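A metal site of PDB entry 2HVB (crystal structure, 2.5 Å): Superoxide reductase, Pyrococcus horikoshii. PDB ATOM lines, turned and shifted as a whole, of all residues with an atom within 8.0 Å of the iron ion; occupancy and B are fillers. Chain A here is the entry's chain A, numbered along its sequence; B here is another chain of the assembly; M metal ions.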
ATOM      1  N   TRP A  20     -16.969  -9.289   6.570  1.00  0.00           N
ATOM      2  CA  TRP A  20     -16.316 -10.231   5.660  1.00  0.00           C
ATOM      3  C   TRP A  20     -17.321 -11.185   5.022  1.00  0.00           C
ATOM      4  O   TRP A  20     -17.162 -12.401   5.039  1.00  0.00           O
ATOM      5  CB  TRP A  20     -15.276 -11.026   6.457  1.00  0.00           C
ATOM      6  CG  TRP A  20     -13.988 -11.050   5.742  1.00  0.00           C
ATOM      7  CD1 TRP A  20     -13.234  -9.936   5.306  1.00  0.00           C
ATOM      8  CD2 TRP A  20     -13.300 -12.225   5.235  1.00  0.00           C
ATOM      9  NE1 TRP A  20     -12.147 -10.291   4.581  1.00  0.00           N
ATOM     10  CE2 TRP A  20     -12.177 -11.775   4.505  1.00  0.00           C
ATOM     11  CE3 TRP A  20     -13.553 -13.591   5.325  1.00  0.00           C
ATOM     12  CZ2 TRP A  20     -11.340 -12.681   3.873  1.00  0.00           C
ATOM     13  CZ3 TRP A  20     -12.718 -14.501   4.701  1.00  0.00           C
ATOM     14  CH2 TRP A  20     -11.605 -14.041   3.974  1.00  0.00           C
ATOM     15  N   GLU A  23     -19.119 -11.820   9.311  1.00  0.00           N
ATOM     16  CA  GLU A  23     -18.355 -11.778  10.555  1.00  0.00           C
ATOM     17  C   GLU A  23     -18.022 -10.341  10.938  1.00  0.00           C
ATOM     18  O   GLU A  23     -17.195  -9.678  10.327  1.00  0.00           O
ATOM     19  CB  GLU A  23     -17.058 -12.550  10.326  1.00  0.00           C
ATOM     20  CG  GLU A  23     -16.411 -13.044  11.635  1.00  0.00           C
ATOM     21  CD  GLU A  23     -15.170 -13.849  11.303  1.00  0.00           C
ATOM     22  OE1 GLU A  23     -14.172 -13.262  10.924  1.00  0.00           O
ATOM     23  OE2 GLU A  23     -15.211 -15.073  11.444  1.00  0.00           O
ATOM     24  N   LYS A  24     -18.727  -9.827  11.959  1.00  0.00           N
ATOM     25  CA  LYS A  24     -18.506  -8.437  12.308  1.00  0.00           C
ATOM     26  C   LYS A  24     -17.093  -8.197  12.831  1.00  0.00           C
ATOM     27  O   LYS A  24     -16.628  -8.842  13.775  1.00  0.00           O
ATOM     28  CB  LYS A  24     -19.561  -8.006  13.333  1.00  0.00           C
ATOM     29  CG  LYS A  24     -20.529  -6.988  12.726  1.00  0.00           C
ATOM     30  CD  LYS A  24     -20.868  -5.841  13.680  1.00  0.00           C
ATOM     31  CE  LYS A  24     -19.696  -4.878  13.892  1.00  0.00           C
ATOM     32  NZ  LYS A  24     -19.396  -4.164  12.656  1.00  0.00           N
ATOM     33  N   HIS A  25     -16.442  -7.230  12.205  1.00  0.00           N
ATOM     34  CA  HIS A  25     -15.104  -6.808  12.602  1.00  0.00           C
ATOM     35  C   HIS A  25     -15.072  -5.322  12.975  1.00  0.00           C
ATOM     36  O   HIS A  25     -14.219  -4.888  13.753  1.00  0.00           O
ATOM     37  CB  HIS A  25     -14.082  -7.061  11.483  1.00  0.00           C
ATOM     38  CG  HIS A  25     -13.633  -8.483  11.362  1.00  0.00           C
ATOM     39  ND1 HIS A  25     -14.259  -9.405  10.543  1.00  0.00           N
ATOM     40  CD2 HIS A  25     -12.580  -9.142  11.917  1.00  0.00           C
ATOM     41  CE1 HIS A  25     -13.619 -10.552  10.604  1.00  0.00           C
ATOM     42  NE2 HIS A  25     -12.594 -10.419  11.420  1.00  0.00           N
ATOM     43  N   VAL A  44     -16.289  -5.147  19.588  1.00  0.00           N
ATOM     44  CA  VAL A  44     -16.375  -5.828  18.311  1.00  0.00           C
ATOM     45  C   VAL A  44     -17.339  -7.000  18.477  1.00  0.00           C
ATOM     46  O   VAL A  44     -17.252  -7.739  19.458  1.00  0.00           O
ATOM     47  CB  VAL A  44     -15.000  -6.350  17.845  1.00  0.00           C
ATOM     48  CG1 VAL A  44     -15.163  -7.166  16.565  1.00  0.00           C
ATOM     49  CG2 VAL A  44     -14.053  -5.172  17.612  1.00  0.00           C
ATOM     50  N   HIS A  50     -17.810 -12.186  17.398  1.00  0.00           N
ATOM     51  CA  HIS A  50     -16.708 -12.656  16.578  1.00  0.00           C
ATOM     52  C   HIS A  50     -16.107 -13.900  17.197  1.00  0.00           C
ATOM     53  O   HIS A  50     -16.188 -14.136  18.393  1.00  0.00           O
ATOM     54  CB  HIS A  50     -15.686 -11.524  16.510  1.00  0.00           C
ATOM     55  CG  HIS A  50     -14.534 -11.939  15.625  1.00  0.00           C
ATOM     56  ND1 HIS A  50     -13.457 -12.612  16.104  1.00  0.00           N
ATOM     57  CD2 HIS A  50     -14.324 -11.666  14.266  1.00  0.00           C
ATOM     58  CE1 HIS A  50     -12.618 -12.734  15.056  1.00  0.00           C
ATOM     59  NE2 HIS A  50     -13.110 -12.172  13.942  1.00  0.00           N
ATOM     60  N   PRO A  51     -15.551 -14.773  16.344  1.00  0.00           N
ATOM     61  CA  PRO A  51     -14.835 -15.924  16.850  1.00  0.00           C
ATOM     62  C   PRO A  51     -13.812 -15.490  17.911  1.00  0.00           C
ATOM     63  O   PRO A  51     -13.070 -14.527  17.755  1.00  0.00           O
ATOM     64  CB  PRO A  51     -14.149 -16.603  15.675  1.00  0.00           C
ATOM     65  CG  PRO A  51     -14.871 -16.154  14.408  1.00  0.00           C
ATOM     66  CD  PRO A  51     -15.539 -14.776  14.887  1.00  0.00           C
ATOM     67  N   GLU A  55      -6.737 -19.561  17.710  1.00  0.00           N
ATOM     68  CA  GLU A  55      -6.479 -19.451  16.268  1.00  0.00           C
ATOM     69  C   GLU A  55      -7.132 -18.224  15.642  1.00  0.00           C
ATOM     70  O   GLU A  55      -6.627 -17.692  14.661  1.00  0.00           O
ATOM     71  CB  GLU A  55      -6.995 -20.680  15.535  1.00  0.00           C
ATOM     72  CG  GLU A  55      -6.710 -22.037  16.177  1.00  0.00           C
ATOM     73  CD  GLU A  55      -7.647 -22.362  17.339  1.00  0.00           C
ATOM     74  OE1 GLU A  55      -8.884 -22.238  17.183  1.00  0.00           O
ATOM     75  OE2 GLU A  55      -7.137 -22.758  18.410  1.00  0.00           O
ATOM     76  N   HIS A  56      -8.264 -17.792  16.176  1.00  0.00           N
ATOM     77  CA  HIS A  56      -8.965 -16.645  15.595  1.00  0.00           C
ATOM     78  C   HIS A  56      -9.649 -15.795  16.661  1.00  0.00           C
ATOM     79  O   HIS A  56     -10.443 -16.298  17.461  1.00  0.00           O
ATOM     80  CB  HIS A  56      -9.995 -17.152  14.582  1.00  0.00           C
ATOM     81  CG  HIS A  56     -10.702 -16.067  13.833  1.00  0.00           C
ATOM     82  ND1 HIS A  56     -11.797 -16.315  13.045  1.00  0.00           N
ATOM     83  CD2 HIS A  56     -10.494 -14.731  13.798  1.00  0.00           C
ATOM     84  CE1 HIS A  56     -12.251 -15.171  12.556  1.00  0.00           C
ATOM     85  NE2 HIS A  56     -11.471 -14.194  12.995  1.00  0.00           N
ATOM     86  N   HIS A  57      -9.327 -14.504  16.646  1.00  0.00           N
ATOM     87  CA  HIS A  57      -9.846 -13.582  17.647  1.00  0.00           C
ATOM     88  C   HIS A  57      -9.493 -12.118  17.377  1.00  0.00           C
ATOM     89  O   HIS A  57      -8.712 -11.784  16.488  1.00  0.00           O
ATOM     90  CB  HIS A  57      -9.251 -13.920  19.002  1.00  0.00           C
ATOM     91  CG  HIS A  57      -7.743 -13.956  18.983  1.00  0.00           C
ATOM     92  ND1 HIS A  57      -7.012 -15.129  18.937  1.00  0.00           N
ATOM     93  CD2 HIS A  57      -6.833 -12.948  18.940  1.00  0.00           C
ATOM     94  CE1 HIS A  57      -5.722 -14.836  18.868  1.00  0.00           C
ATOM     95  NE2 HIS A  57      -5.583 -13.529  18.860  1.00  0.00           N
ATOM     96  N   ILE A  58     -10.098 -11.248  18.162  1.00  0.00           N
ATOM     97  CA  ILE A  58      -9.830  -9.824  18.087  1.00  0.00           C
ATOM     98  C   ILE A  58      -8.737  -9.685  19.184  1.00  0.00           C
ATOM     99  O   ILE A  58      -8.971 -10.053  20.348  1.00  0.00           O
ATOM    100  CB  ILE A  58     -11.057  -8.994  18.463  1.00  0.00           C
ATOM    101  CG1 ILE A  58     -12.210  -9.373  17.524  1.00  0.00           C
ATOM    102  CG2 ILE A  58     -10.724  -7.523  18.399  1.00  0.00           C
ATOM    103  CD1 ILE A  58     -12.006  -9.078  16.051  1.00  0.00           C
ATOM    104  N   TYR A 110      -7.905  -4.937  15.689  1.00  0.00           N
ATOM    105  CA  TYR A 110      -7.125  -5.880  14.908  1.00  0.00           C
ATOM    106  C   TYR A 110      -7.508  -7.344  15.127  1.00  0.00           C
ATOM    107  O   TYR A 110      -7.524  -7.835  16.254  1.00  0.00           O
ATOM    108  CB  TYR A 110      -5.644  -5.680  15.224  1.00  0.00           C
ATOM    109  CG  TYR A 110      -4.732  -6.713  14.606  1.00  0.00           C
ATOM    110  CD1 TYR A 110      -4.373  -6.642  13.251  1.00  0.00           C
ATOM    111  CD2 TYR A 110      -4.271  -7.796  15.350  1.00  0.00           C
ATOM    112  CE1 TYR A 110      -3.588  -7.642  12.669  1.00  0.00           C
ATOM    113  CE2 TYR A 110      -3.497  -8.789  14.779  1.00  0.00           C
ATOM    114  CZ  TYR A 110      -3.161  -8.713  13.442  1.00  0.00           C
ATOM    115  OH  TYR A 110      -2.401  -9.711  12.888  1.00  0.00           O
ATOM    116  N   CYS A 111      -7.817  -8.043  14.031  1.00  0.00           N
ATOM    117  CA  CYS A 111      -8.136  -9.465  14.106  1.00  0.00           C
ATOM    118  C   CYS A 111      -6.868 -10.195  13.689  1.00  0.00           C
ATOM    119  O   CYS A 111      -6.239  -9.864  12.685  1.00  0.00           O
ATOM    120  CB  CYS A 111      -9.270  -9.823  13.135  1.00  0.00           C
ATOM    121  SG  CYS A 111      -9.635 -11.599  13.076  1.00  0.00           S
ATOM    122  N   ASN A 112      -6.475 -11.217  14.451  1.00  0.00           N
ATOM    123  CA  ASN A 112      -5.254 -11.937  14.125  1.00  0.00           C
ATOM    124  C   ASN A 112      -5.201 -12.531  12.718  1.00  0.00           C
ATOM    125  O   ASN A 112      -4.121 -12.782  12.195  1.00  0.00           O
ATOM    126  CB  ASN A 112      -4.976 -13.005  15.181  1.00  0.00           C
ATOM    127  CG  ASN A 112      -5.967 -14.131  15.150  1.00  0.00           C
ATOM    128  OD1 ASN A 112      -7.175 -13.910  15.213  1.00  0.00           O
ATOM    129  ND2 ASN A 112      -5.459 -15.360  15.050  1.00  0.00           N
ATOM    130  N   ILE A 113      -6.356 -12.762  12.086  1.00  0.00           N
ATOM    131  CA  ILE A 113      -6.329 -13.320  10.730  1.00  0.00           C
ATOM    132  C   ILE A 113      -7.046 -12.482   9.677  1.00  0.00           C
ATOM    133  O   ILE A 113      -7.030 -12.833   8.506  1.00  0.00           O
ATOM    134  CB  ILE A 113      -6.925 -14.769  10.683  1.00  0.00           C
ATOM    135  CG1 ILE A 113      -8.420 -14.741  10.943  1.00  0.00           C
ATOM    136  CG2 ILE A 113      -6.251 -15.652  11.720  1.00  0.00           C
ATOM    137  CD1 ILE A 113      -9.069 -16.115  10.792  1.00  0.00           C
ATOM    138  N   HIS A 114      -7.661 -11.371  10.090  1.00  0.00           N
ATOM    139  CA  HIS A 114      -8.366 -10.493   9.154  1.00  0.00           C
ATOM    140  C   HIS A 114      -7.885  -9.036   9.164  1.00  0.00           C
ATOM    141  O   HIS A 114      -8.586  -8.133   8.688  1.00  0.00           O
ATOM    142  CB  HIS A 114      -9.864 -10.555   9.423  1.00  0.00           C
ATOM    143  CG  HIS A 114     -10.447 -11.910   9.163  1.00  0.00           C
ATOM    144  ND1 HIS A 114     -11.251 -12.556  10.083  1.00  0.00           N
ATOM    145  CD2 HIS A 114     -10.329 -12.750   8.107  1.00  0.00           C
ATOM    146  CE1 HIS A 114     -11.597 -13.740   9.605  1.00  0.00           C
ATOM    147  NE2 HIS A 114     -11.059 -13.879   8.412  1.00  0.00           N
ATOM    148  N   GLY A 115      -6.690  -8.810   9.694  1.00  0.00           N
ATOM    149  CA  GLY A 115      -6.133  -7.477   9.710  1.00  0.00           C
ATOM    150  C   GLY A 115      -6.833  -6.376  10.493  1.00  0.00           C
ATOM    151  O   GLY A 115      -7.577  -6.623  11.458  1.00  0.00           O
ATOM    152  N   TRP A 117      -9.187  -2.913  11.208  1.00  0.00           N
ATOM    153  CA  TRP A 117     -10.527  -2.366  11.001  1.00  0.00           C
ATOM    154  C   TRP A 117     -10.662  -1.052  11.751  1.00  0.00           C
ATOM    155  O   TRP A 117     -10.146  -0.906  12.864  1.00  0.00           O
ATOM    156  CB  TRP A 117     -11.601  -3.334  11.481  1.00  0.00           C
ATOM    157  CG  TRP A 117     -11.600  -4.585  10.667  1.00  0.00           C
ATOM    158  CD1 TRP A 117     -10.703  -5.602  10.753  1.00  0.00           C
ATOM    159  CD2 TRP A 117     -12.441  -4.877   9.551  1.00  0.00           C
ATOM    160  NE1 TRP A 117     -10.924  -6.517   9.761  1.00  0.00           N
ATOM    161  CE2 TRP A 117     -11.986  -6.091   9.006  1.00  0.00           C
ATOM    162  CE3 TRP A 117     -13.527  -4.222   8.954  1.00  0.00           C
ATOM    163  CZ2 TRP A 117     -12.593  -6.679   7.879  1.00  0.00           C
ATOM    164  CZ3 TRP A 117     -14.133  -4.801   7.830  1.00  0.00           C
ATOM    165  CH2 TRP A 117     -13.653  -6.025   7.308  1.00  0.00           C
ATOM    166  N   PHE B  72      -4.604 -10.327   3.893  1.00  0.00           N
ATOM    167  CA  PHE B  72      -4.470  -9.441   5.051  1.00  0.00           C
ATOM    168  C   PHE B  72      -3.065  -9.368   5.618  1.00  0.00           C
ATOM    169  O   PHE B  72      -2.323 -10.342   5.584  1.00  0.00           O
ATOM    170  CB  PHE B  72      -5.381  -9.888   6.162  1.00  0.00           C
ATOM    171  CG  PHE B  72      -6.774 -10.041   5.743  1.00  0.00           C
ATOM    172  CD1 PHE B  72      -7.515  -8.927   5.392  1.00  0.00           C
ATOM    173  CD2 PHE B  72      -7.371 -11.283   5.775  1.00  0.00           C
ATOM    174  CE1 PHE B  72      -8.852  -9.056   5.072  1.00  0.00           C
ATOM    175  CE2 PHE B  72      -8.699 -11.423   5.453  1.00  0.00           C
ATOM    176  CZ  PHE B  72      -9.432 -10.305   5.116  1.00  0.00           C
HETATM  177 FE    FE M   1     -11.627 -12.184  12.150  1.00  0.00          FE
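Residues that only touch the iron ion: Glu 23.
Along chain A the residues within 4 Å of the iron ion span positions 23 to 114.
The nearest printed residue that does not touch the iron ion is Ile 113 (4.3 Å).
The iron ion is bound by ND1 of His 114, NE2 of His 25, NE2 of His 56, SG of Cys 111 and NE2 of His 50.
The iron ion has five donor atoms within binding distance.
The indole nitrogen of Trp 117 sits at hydrogen-bond distance from the backbone carbonyl oxygen of His 114, 3.0 Å away.
The side-chain carboxylate of Glu 23 lies close to a ring nitrogen (ND1) of His 114, 3.1 Å away.
The backbone carbonyl oxygen of Glu 23 is in hydrogen-bond range of a ring nitrogen (ND1) of His 25 (3.0 Å).
The backbone carbonyl oxygen (O) of His 57 lies close to the side-chain sulfur (SG) of Cys 111 (3.5 Å).
A ring nitrogen (NE2) of His 50 lies close to the side-chain carboxylate of Glu 23 (3.4 Å).
N of Ile 113 sits close to SG of Cys 111 (3.6 Å).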
